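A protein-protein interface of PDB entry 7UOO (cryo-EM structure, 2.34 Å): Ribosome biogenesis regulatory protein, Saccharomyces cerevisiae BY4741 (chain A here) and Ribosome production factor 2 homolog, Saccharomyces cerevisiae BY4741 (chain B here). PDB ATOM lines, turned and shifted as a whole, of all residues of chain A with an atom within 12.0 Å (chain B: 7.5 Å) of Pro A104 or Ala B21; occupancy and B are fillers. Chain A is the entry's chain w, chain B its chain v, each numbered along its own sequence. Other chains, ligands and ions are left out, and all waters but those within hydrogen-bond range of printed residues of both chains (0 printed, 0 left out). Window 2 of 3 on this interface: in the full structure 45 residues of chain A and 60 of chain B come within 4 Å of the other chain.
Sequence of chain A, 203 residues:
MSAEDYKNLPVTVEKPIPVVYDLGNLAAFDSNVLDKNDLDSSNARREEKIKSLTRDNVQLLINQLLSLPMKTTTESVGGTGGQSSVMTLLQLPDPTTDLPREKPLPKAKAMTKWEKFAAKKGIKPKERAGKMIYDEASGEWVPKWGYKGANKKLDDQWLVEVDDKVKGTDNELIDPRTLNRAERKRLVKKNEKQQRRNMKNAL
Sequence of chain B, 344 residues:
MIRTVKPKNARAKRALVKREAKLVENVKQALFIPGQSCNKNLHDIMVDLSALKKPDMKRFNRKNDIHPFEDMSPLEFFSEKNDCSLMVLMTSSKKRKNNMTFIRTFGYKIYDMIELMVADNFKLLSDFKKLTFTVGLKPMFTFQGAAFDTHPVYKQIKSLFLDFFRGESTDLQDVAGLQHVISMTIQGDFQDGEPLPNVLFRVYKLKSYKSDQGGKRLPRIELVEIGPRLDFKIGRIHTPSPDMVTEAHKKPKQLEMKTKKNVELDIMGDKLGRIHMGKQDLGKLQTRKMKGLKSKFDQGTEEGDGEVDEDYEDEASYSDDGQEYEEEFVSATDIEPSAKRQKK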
ATOM      1  N   LEU A  99     -15.112   9.139   9.331  1.00  0.00           N
ATOM      2  CA  LEU A  99     -16.366   8.511   9.704  1.00  0.00           C
ATOM      3  C   LEU A  99     -16.677   7.379   8.738  1.00  0.00           C
ATOM      4  O   LEU A  99     -16.338   7.461   7.553  1.00  0.00           O
ATOM      5  CB  LEU A  99     -17.519   9.525   9.696  1.00  0.00           C
ATOM      6  CG  LEU A  99     -17.386  10.723  10.636  1.00  0.00           C
ATOM      7  CD1 LEU A  99     -18.573  11.656  10.479  1.00  0.00           C
ATOM      8  CD2 LEU A  99     -17.256  10.261  12.074  1.00  0.00           C
ATOM      9  N   PRO A 100     -17.309   6.310   9.216  1.00  0.00           N
ATOM     10  CA  PRO A 100     -17.664   5.206   8.320  1.00  0.00           C
ATOM     11  C   PRO A 100     -18.723   5.614   7.310  1.00  0.00           C
ATOM     12  O   PRO A 100     -19.571   6.471   7.570  1.00  0.00           O
ATOM     13  CB  PRO A 100     -18.192   4.131   9.275  1.00  0.00           C
ATOM     14  CG  PRO A 100     -18.643   4.884  10.476  1.00  0.00           C
ATOM     15  CD  PRO A 100     -17.686   6.028  10.611  1.00  0.00           C
ATOM     16  N   ARG A 101     -18.660   4.988   6.140  1.00  0.00           N
ATOM     17  CA  ARG A 101     -19.655   5.219   5.107  1.00  0.00           C
ATOM     18  C   ARG A 101     -20.959   4.509   5.456  1.00  0.00           C
ATOM     19  O   ARG A 101     -21.012   3.641   6.331  1.00  0.00           O
ATOM     20  CB  ARG A 101     -19.148   4.732   3.748  1.00  0.00           C
ATOM     21  CG  ARG A 101     -17.847   5.366   3.297  1.00  0.00           C
ATOM     22  CD  ARG A 101     -17.992   5.992   1.925  1.00  0.00           C
ATOM     23  NE  ARG A 101     -18.585   5.072   0.963  1.00  0.00           N
ATOM     24  CZ  ARG A 101     -18.922   5.400  -0.277  1.00  0.00           C
ATOM     25  NH1 ARG A 101     -18.728   6.622  -0.745  1.00  0.00           N
ATOM     26  NH2 ARG A 101     -19.471   4.480  -1.065  1.00  0.00           N
ATOM     27  N   GLU A 102     -22.027   4.898   4.762  1.00  0.00           N
ATOM     28  CA  GLU A 102     -23.304   4.214   4.899  1.00  0.00           C
ATOM     29  C   GLU A 102     -23.450   3.044   3.940  1.00  0.00           C
ATOM     30  O   GLU A 102     -24.217   2.117   4.225  1.00  0.00           O
ATOM     31  CB  GLU A 102     -24.460   5.196   4.687  1.00  0.00           C
ATOM     32  CG  GLU A 102     -24.371   5.998   3.401  1.00  0.00           C
ATOM     33  CD  GLU A 102     -25.550   6.933   3.222  1.00  0.00           C
ATOM     34  OE1 GLU A 102     -26.560   6.759   3.935  1.00  0.00           O
ATOM     35  OE2 GLU A 102     -25.466   7.843   2.371  1.00  0.00           O
ATOM     36  N   LYS A 103     -22.734   3.062   2.821  1.00  0.00           N
ATOM     37  CA  LYS A 103     -22.768   2.003   1.827  1.00  0.00           C
ATOM     38  C   LYS A 103     -21.362   1.775   1.297  1.00  0.00           C
ATOM     39  O   LYS A 103     -20.541   2.701   1.293  1.00  0.00           O
ATOM     40  CB  LYS A 103     -23.715   2.353   0.667  1.00  0.00           C
ATOM     41  CG  LYS A 103     -25.178   2.085   0.967  1.00  0.00           C
ATOM     42  CD  LYS A 103     -26.063   2.574  -0.161  1.00  0.00           C
ATOM     43  CE  LYS A 103     -25.960   4.078  -0.314  1.00  0.00           C
ATOM     44  NZ  LYS A 103     -26.373   4.786   0.927  1.00  0.00           N
ATOM     45  N   PRO A 104     -21.051   0.559   0.852  1.00  0.00           N
ATOM     46  CA  PRO A 104     -19.720   0.299   0.296  1.00  0.00           C
ATOM     47  C   PRO A 104     -19.535   0.979  -1.051  1.00  0.00           C
ATOM     48  O   PRO A 104     -20.490   1.402  -1.706  1.00  0.00           O
ATOM     49  CB  PRO A 104     -19.686  -1.226   0.158  1.00  0.00           C
ATOM     50  CG  PRO A 104     -21.113  -1.620   0.036  1.00  0.00           C
ATOM     51  CD  PRO A 104     -21.867  -0.666   0.915  1.00  0.00           C
ATOM     52  N   LEU A 105     -18.271   1.087  -1.453  1.00  0.00           N
ATOM     53  CA  LEU A 105     -17.936   1.699  -2.728  1.00  0.00           C
ATOM     54  C   LEU A 105     -18.482   0.860  -3.882  1.00  0.00           C
ATOM     55  O   LEU A 105     -18.562  -0.368  -3.784  1.00  0.00           O
ATOM     56  CB  LEU A 105     -16.423   1.849  -2.869  1.00  0.00           C
ATOM     57  CG  LEU A 105     -15.739   2.958  -2.073  1.00  0.00           C
ATOM     58  CD1 LEU A 105     -14.246   2.929  -2.335  1.00  0.00           C
ATOM     59  CD2 LEU A 105     -16.318   4.311  -2.438  1.00  0.00           C
ATOM     60  N   PRO A 106     -18.877   1.499  -4.984  1.00  0.00           N
ATOM     61  CA  PRO A 106     -19.386   0.747  -6.143  1.00  0.00           C
ATOM     62  C   PRO A 106     -18.283  -0.088  -6.776  1.00  0.00           C
ATOM     63  O   PRO A 106     -17.241   0.434  -7.174  1.00  0.00           O
ATOM     64  CB  PRO A 106     -19.879   1.847  -7.091  1.00  0.00           C
ATOM     65  CG  PRO A 106     -20.070   3.049  -6.223  1.00  0.00           C
ATOM     66  CD  PRO A 106     -19.018   2.952  -5.168  1.00  0.00           C
ATOM     67  N   LYS A 107     -18.521  -1.395  -6.862  1.00  0.00           N
ATOM     68  CA  LYS A 107     -17.546  -2.309  -7.436  1.00  0.00           C
ATOM     69  C   LYS A 107     -17.379  -2.066  -8.932  1.00  0.00           C
ATOM     70  O   LYS A 107     -18.315  -1.667  -9.631  1.00  0.00           O
ATOM     71  CB  LYS A 107     -17.967  -3.757  -7.193  1.00  0.00           C
ATOM     72  CG  LYS A 107     -17.866  -4.206  -5.745  1.00  0.00           C
ATOM     73  CD  LYS A 107     -18.394  -5.622  -5.571  1.00  0.00           C
ATOM     74  CE  LYS A 107     -17.753  -6.583  -6.562  1.00  0.00           C
ATOM     75  NZ  LYS A 107     -16.274  -6.645  -6.411  1.00  0.00           N
ATOM     76  N   ALA A 108     -16.168  -2.316  -9.421  1.00  0.00           N
ATOM     77  CA  ALA A 108     -15.898  -2.207 -10.848  1.00  0.00           C
ATOM     78  C   ALA A 108     -16.509  -3.398 -11.573  1.00  0.00           C
ATOM     79  O   ALA A 108     -16.171  -4.550 -11.285  1.00  0.00           O
ATOM     80  CB  ALA A 108     -14.394  -2.133 -11.099  1.00  0.00           C
ATOM     81  N   LYS A 109     -17.415  -3.120 -12.507  1.00  0.00           N
ATOM     82  CA  LYS A 109     -18.111  -4.184 -13.218  1.00  0.00           C
ATOM     83  C   LYS A 109     -17.153  -4.935 -14.133  1.00  0.00           C
ATOM     84  O   LYS A 109     -16.322  -4.334 -14.820  1.00  0.00           O
ATOM     85  CB  LYS A 109     -19.272  -3.606 -14.026  1.00  0.00           C
ATOM     86  CG  LYS A 109     -20.142  -4.650 -14.714  1.00  0.00           C
ATOM     87  CD  LYS A 109     -20.794  -5.595 -13.712  1.00  0.00           C
ATOM     88  CE  LYS A 109     -21.696  -4.846 -12.742  1.00  0.00           C
ATOM     89  NZ  LYS A 109     -22.472  -5.771 -11.872  1.00  0.00           N
ATOM     90  N   LEU B  16     -34.622   4.243  -7.147  1.00  0.00           N
ATOM     91  CA  LEU B  16     -33.578   3.229  -7.024  1.00  0.00           C
ATOM     92  C   LEU B  16     -32.189   3.827  -7.231  1.00  0.00           C
ATOM     93  O   LEU B  16     -31.237   3.462  -6.530  1.00  0.00           O
ATOM     94  CB  LEU B  16     -33.823   2.093  -8.017  1.00  0.00           C
ATOM     95  CG  LEU B  16     -34.971   1.137  -7.694  1.00  0.00           C
ATOM     96  CD1 LEU B  16     -35.007  -0.013  -8.688  1.00  0.00           C
ATOM     97  CD2 LEU B  16     -34.854   0.618  -6.271  1.00  0.00           C
ATOM     98  N   VAL B  17     -32.053   4.739  -8.198  1.00  0.00           N
ATOM     99  CA  VAL B  17     -30.768   5.391  -8.445  1.00  0.00           C
ATOM    100  C   VAL B  17     -30.358   6.237  -7.247  1.00  0.00           C
ATOM    101  O   VAL B  17     -29.188   6.248  -6.842  1.00  0.00           O
ATOM    102  CB  VAL B  17     -30.837   6.223  -9.740  1.00  0.00           C
ATOM    103  CG1 VAL B  17     -29.654   7.169  -9.844  1.00  0.00           C
ATOM    104  CG2 VAL B  17     -30.881   5.305 -10.950  1.00  0.00           C
ATOM    105  N   LYS B  18     -31.315   6.955  -6.656  1.00  0.00           N
ATOM    106  CA  LYS B  18     -31.031   7.735  -5.456  1.00  0.00           C
ATOM    107  C   LYS B  18     -30.630   6.834  -4.294  1.00  0.00           C
ATOM    108  O   LYS B  18     -29.775   7.200  -3.479  1.00  0.00           O
ATOM    109  CB  LYS B  18     -32.251   8.578  -5.092  1.00  0.00           C
ATOM    110  CG  LYS B  18     -32.028   9.570  -3.972  1.00  0.00           C
ATOM    111  CD  LYS B  18     -33.287  10.381  -3.713  1.00  0.00           C
ATOM    112  CE  LYS B  18     -33.791  11.047  -4.989  1.00  0.00           C
ATOM    113  NZ  LYS B  18     -35.009  11.863  -4.742  1.00  0.00           N
ATOM    114  N   ARG B  19     -31.235   5.650  -4.205  1.00  0.00           N
ATOM    115  CA  ARG B  19     -30.935   4.740  -3.107  1.00  0.00           C
ATOM    116  C   ARG B  19     -29.587   4.045  -3.273  1.00  0.00           C
ATOM    117  O   ARG B  19     -28.926   3.747  -2.272  1.00  0.00           O
ATOM    118  CB  ARG B  19     -32.052   3.703  -2.979  1.00  0.00           C
ATOM    119  CG  ARG B  19     -31.966   2.846  -1.737  1.00  0.00           C
ATOM    120  CD  ARG B  19     -33.331   2.316  -1.341  1.00  0.00           C
ATOM    121  NE  ARG B  19     -34.315   3.388  -1.238  1.00  0.00           N
ATOM    122  CZ  ARG B  19     -35.493   3.268  -0.641  1.00  0.00           C
ATOM    123  NH1 ARG B  19     -35.859   2.140  -0.054  1.00  0.00           N
ATOM    124  NH2 ARG B  19     -36.323   4.307  -0.630  1.00  0.00           N
ATOM    125  N   GLU B  20     -29.163   3.786  -4.507  1.00  0.00           N
ATOM    126  CA  GLU B  20     -27.945   3.017  -4.727  1.00  0.00           C
ATOM    127  C   GLU B  20     -26.707   3.810  -4.307  1.00  0.00           C
ATOM    128  O   GLU B  20     -26.741   5.030  -4.129  1.00  0.00           O
ATOM    129  CB  GLU B  20     -27.828   2.599  -6.193  1.00  0.00           C
ATOM    130  CG  GLU B  20     -27.270   3.668  -7.114  1.00  0.00           C
ATOM    131  CD  GLU B  20     -27.332   3.262  -8.575  1.00  0.00           C
ATOM    132  OE1 GLU B  20     -27.850   2.165  -8.865  1.00  0.00           O
ATOM    133  OE2 GLU B  20     -26.863   4.040  -9.433  1.00  0.00           O
ATOM    134  N   ALA B  21     -25.603   3.086  -4.140  1.00  0.00           N
ATOM    135  CA  ALA B  21     -24.368   3.676  -3.645  1.00  0.00           C
ATOM    136  C   ALA B  21     -23.741   4.601  -4.681  1.00  0.00           C
ATOM    137  O   ALA B  21     -23.924   4.436  -5.891  1.00  0.00           O
ATOM    138  CB  ALA B  21     -23.373   2.585  -3.257  1.00  0.00           C
ATOM    139  N   LYS B  22     -22.981   5.578  -4.191  1.00  0.00           N
ATOM    140  CA  LYS B  22     -22.346   6.566  -5.049  1.00  0.00           C
ATOM    141  C   LYS B  22     -21.043   7.019  -4.406  1.00  0.00           C
ATOM    142  O   LYS B  22     -20.793   6.772  -3.223  1.00  0.00           O
ATOM    143  CB  LYS B  22     -23.277   7.755  -5.309  1.00  0.00           C
ATOM    144  CG  LYS B  22     -23.886   8.350  -4.055  1.00  0.00           C
ATOM    145  CD  LYS B  22     -25.146   9.138  -4.376  1.00  0.00           C
ATOM    146  CE  LYS B  22     -26.214   8.235  -4.971  1.00  0.00           C
ATOM    147  NZ  LYS B  22     -27.501   8.947  -5.188  1.00  0.00           N
ATOM    148  N   LEU B  23     -20.206   7.676  -5.213  1.00  0.00           N
ATOM    149  CA  LEU B  23     -18.885   8.092  -4.748  1.00  0.00           C
ATOM    150  C   LEU B  23     -18.980   9.134  -3.638  1.00  0.00           C
ATOM    151  O   LEU B  23     -18.240   9.063  -2.650  1.00  0.00           O
ATOM    152  CB  LEU B  23     -18.064   8.626  -5.921  1.00  0.00           C
ATOM    153  CG  LEU B  23     -17.821   7.637  -7.062  1.00  0.00           C
ATOM    154  CD1 LEU B  23     -17.045   8.296  -8.189  1.00  0.00           C
ATOM    155  CD2 LEU B  23     -17.088   6.408  -6.555  1.00  0.00           C
ATOM    156  N   VAL B  24     -19.871  10.109  -3.784  1.00  0.00           N
ATOM    157  CA  VAL B  24     -20.128  11.112  -2.755  1.00  0.00           C
ATOM    158  C   VAL B  24     -21.502  10.811  -2.173  1.00  0.00           C
ATOM    159  O   VAL B  24     -22.527  11.063  -2.816  1.00  0.00           O
ATOM    160  CB  VAL B  24     -20.059  12.540  -3.312  1.00  0.00           C
ATOM    161  CG1 VAL B  24     -20.400  13.548  -2.230  1.00  0.00           C
ATOM    162  CG2 VAL B  24     -18.680  12.817  -3.885  1.00  0.00           C
ATOM    163  N   GLU B  25     -21.525  10.273  -0.957  1.00  0.00           N
ATOM    164  CA  GLU B  25     -22.762   9.794  -0.363  1.00  0.00           C
ATOM    165  C   GLU B  25     -23.638  10.950   0.112  1.00  0.00           C
ATOM    166  O   GLU B  25     -23.168  12.057   0.386  1.00  0.00           O
ATOM    167  CB  GLU B  25     -22.470   8.848   0.801  1.00  0.00           C
ATOM    168  CG  GLU B  25     -21.973   7.470   0.379  1.00  0.00           C
ATOM    169  CD  GLU B  25     -23.037   6.649  -0.336  1.00  0.00           C
ATOM    170  OE1 GLU B  25     -24.239   6.961  -0.194  1.00  0.00           O
ATOM    171  OE2 GLU B  25     -22.669   5.686  -1.041  1.00  0.00           O
ATOM    172  N   PHE B 106     -24.015  -0.271   8.085  1.00  0.00           N
ATOM    173  CA  PHE B 106     -23.156  -0.176   6.912  1.00  0.00           C
ATOM    174  C   PHE B 106     -23.599  -1.220   5.898  1.00  0.00           C
ATOM    175  O   PHE B 106     -23.561  -2.420   6.186  1.00  0.00           O
ATOM    176  CB  PHE B 106     -21.685  -0.375   7.286  1.00  0.00           C
ATOM    177  CG  PHE B 106     -20.762  -0.455   6.105  1.00  0.00           C
ATOM    178  CD1 PHE B 106     -20.424   0.684   5.395  1.00  0.00           C
ATOM    179  CD2 PHE B 106     -20.221  -1.667   5.712  1.00  0.00           C
ATOM    180  CE1 PHE B 106     -19.574   0.615   4.310  1.00  0.00           C
ATOM    181  CE2 PHE B 106     -19.367  -1.742   4.630  1.00  0.00           C
ATOM    182  CZ  PHE B 106     -19.043  -0.599   3.928  1.00  0.00           C
ATOM    183  N   GLY B 107     -24.005  -0.763   4.717  1.00  0.00           N
ATOM    184  CA  GLY B 107     -24.485  -1.668   3.682  1.00  0.00           C
ATOM    185  C   GLY B 107     -25.739  -2.421   4.065  1.00  0.00           C
ATOM    186  O   GLY B 107     -25.860  -3.614   3.760  1.00  0.00           O
ATOM    187  N   TYR B 108     -26.673  -1.748   4.746  1.00  0.00           N
ATOM    188  CA  TYR B 108     -27.910  -2.330   5.268  1.00  0.00           C
ATOM    189  C   TYR B 108     -27.650  -3.473   6.247  1.00  0.00           C
ATOM    190  O   TYR B 108     -28.526  -4.311   6.478  1.00  0.00           O
ATOM    191  CB  TYR B 108     -28.840  -2.790   4.137  1.00  0.00           C
ATOM    192  CG  TYR B 108     -29.342  -1.652   3.282  1.00  0.00           C
ATOM    193  CD1 TYR B 108     -29.523  -0.385   3.823  1.00  0.00           C
ATOM    194  CD2 TYR B 108     -29.626  -1.837   1.935  1.00  0.00           C
ATOM    195  CE1 TYR B 108     -29.977   0.662   3.052  1.00  0.00           C
ATOM    196  CE2 TYR B 108     -30.080  -0.792   1.153  1.00  0.00           C
ATOM    197  CZ  TYR B 108     -30.254   0.456   1.720  1.00  0.00           C
ATOM    198  OH  TYR B 108     -30.706   1.504   0.955  1.00  0.00           O
ATOM    199  N   GLU B 247     -13.524  -1.625   5.276  1.00  0.00           N
ATOM    200  CA  GLU B 247     -14.432  -1.451   4.146  1.00  0.00           C
ATOM    201  C   GLU B 247     -15.236  -0.161   4.273  1.00  0.00           C
ATOM    202  O   GLU B 247     -15.495   0.518   3.274  1.00  0.00           O
ATOM    203  CB  GLU B 247     -15.363  -2.658   4.029  1.00  0.00           C
ATOM    204  CG  GLU B 247     -16.193  -2.678   2.755  1.00  0.00           C
ATOM    205  CD  GLU B 247     -17.026  -3.940   2.610  1.00  0.00           C
ATOM    206  OE1 GLU B 247     -17.419  -4.523   3.644  1.00  0.00           O
ATOM    207  OE2 GLU B 247     -17.282  -4.352   1.459  1.00  0.00           O
ATOM    208  N   ALA B 248     -15.639   0.192   5.494  1.00  0.00           N
ATOM    209  CA  ALA B 248     -16.379   1.425   5.720  1.00  0.00           C
ATOM    210  C   ALA B 248     -15.497   2.663   5.667  1.00  0.00           C
ATOM    211  O   ALA B 248     -16.016   3.766   5.465  1.00  0.00           O
ATOM    212  CB  ALA B 248     -17.097   1.365   7.069  1.00  0.00           C
ATOM    213  N   LYS B 250     -12.795   2.839   3.515  1.00  0.00           N
ATOM    214  CA  LYS B 250     -12.212   2.969   2.184  1.00  0.00           C
ATOM    215  C   LYS B 250     -12.684   4.255   1.509  1.00  0.00           C
ATOM    216  O   LYS B 250     -13.786   4.749   1.761  1.00  0.00           O
ATOM    217  CB  LYS B 250     -12.576   1.763   1.316  1.00  0.00           C
ATOM    218  CG  LYS B 250     -11.717   0.529   1.551  1.00  0.00           C
ATOM    219  CD  LYS B 250     -12.060  -0.571   0.555  1.00  0.00           C
ATOM    220  CE  LYS B 250     -11.036  -1.696   0.589  1.00  0.00           C
ATOM    221  NZ  LYS B 250     -11.015  -2.416   1.895  1.00  0.00           N
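Pro A100 touches Ala B248 (CA to O, 3.6 Å). O of Arg A101 touches CD1 of Phe B106 (3.2 Å). O of Glu A102 touches CA of Phe B106, at 3.7 Å. Arg B19 touches Lys A103. Ala B21 touches Lys A103. C of Lys A103 touches CE1 of Phe B106, at 3.7 Å. O of Pro A104 touches CB of Ala B21, 3.5 Å away. N of Pro A104 touches CE1 of Phe B106 (3.8 Å). CD of Pro A104 touches CA of Gly B107, at 3.9 Å.
Of the printed residues of chain B, Glu A102 touches Glu B25, Phe B106 and Gly B107. Of the printed residues of chain B, Lys A103 touches Arg B19 (3.6 Å), Ala B21 (3.7 Å), Glu B25 (3.2 Å) and Phe B106 (3.7 Å). Pro A104 touches just these residues of chain B: Ala B21, Phe B106 and Gly B107. Printed residues of chain A within 4 Å of Arg B19: Lys A103. Of chain A, only Lys A103 (3.7 Å) and Pro A104 (3.5 Å) come within 4 Å of Ala B21. Printed residues of chain A within 4 Å of Lys B22: Arg A101 (3.2 Å). Of the printed residues of chain A, Leu B23 touches Arg A101 (3.1 Å). Of the printed residues of chain A, Glu B25 touches Arg A101, Glu A102 and Lys A103. Phe B106 touches four residues of chain A. The nearest residue of chain A that does not touch Ala B21 is Pro A106 (4.1 Å). The nearest printed residue of chain B that does not touch Pro A100 is Phe B106 (5.6 Å).
The backbone carbonyl oxygen of Lys B18 is in hydrogen-bond range of the side-chain amino group of Lys B22 (3.3 Å). The side-chain carboxylate of Glu B25 sits at hydrogen-bond distance from the backbone NH of Lys B22, at 3.2 Å. NE of Arg A101 lies within hydrogen-bond range of O of Lys A103 (3.1 Å). The guanidinium group (NH2) of Arg A101 is in hydrogen-bond range of the backbone carbonyl oxygen (O) of Pro A104 (3.3 Å). The side-chain carboxylate of Glu A102 lies within salt-bridge range of the side-chain amino group of Lys A103 (3.5 Å).
Printed residues of chain A that touch a printed residue of chain B: Pro A100, Arg A101, Glu A102, Lys A103 and Pro A104. Hydrophobic or aromatic side chains of chain A within 4 Å of the printed part of chain B: Pro A100 and Pro A104. Printed residues of chain B that touch a printed residue of chain A: Arg B19, Ala B21, Lys B22, Leu B23, Glu B25, Phe B106, Gly B107 and Ala B248. Among the printed residues, 16 pairs touch across the chains. Among the printed residues, Asp or Glu carboxylates within 4 Å of a Lys or Arg side-chain nitrogen of the other chain: Arg A101 with Glu B25 (3.4 Å) and Lys A103 with Glu B25 (3.2 Å).
NH1 of Arg A101 is in hydrogen-bond range of O of Lys B22, at 3.2 Å. The backbone carbonyl oxygen of Leu B23 sits at hydrogen-bond distance from the guanidinium group of Arg A101, at 3.1 Å. The side-chain carboxylate (OE2) of Glu B25 lies within salt-bridge range of the guanidinium group (NH2) of Arg A101 (3.4 Å). The side-chain amino group (NZ) of Lys A103 lies within salt-bridge range of the side-chain carboxylate (OE1) of Glu B25. N of Gly B107 lies within hydrogen-bond range of O of Glu A102 (2.9 Å). The backbone carbonyl oxygen (O) of Ala B248 lies within hydrogen-bond range of the backbone NH (N) of Arg A101 (3.0 Å). OE1 of Glu B25 lies close to OE2 of Glu A102 (3.0 Å).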
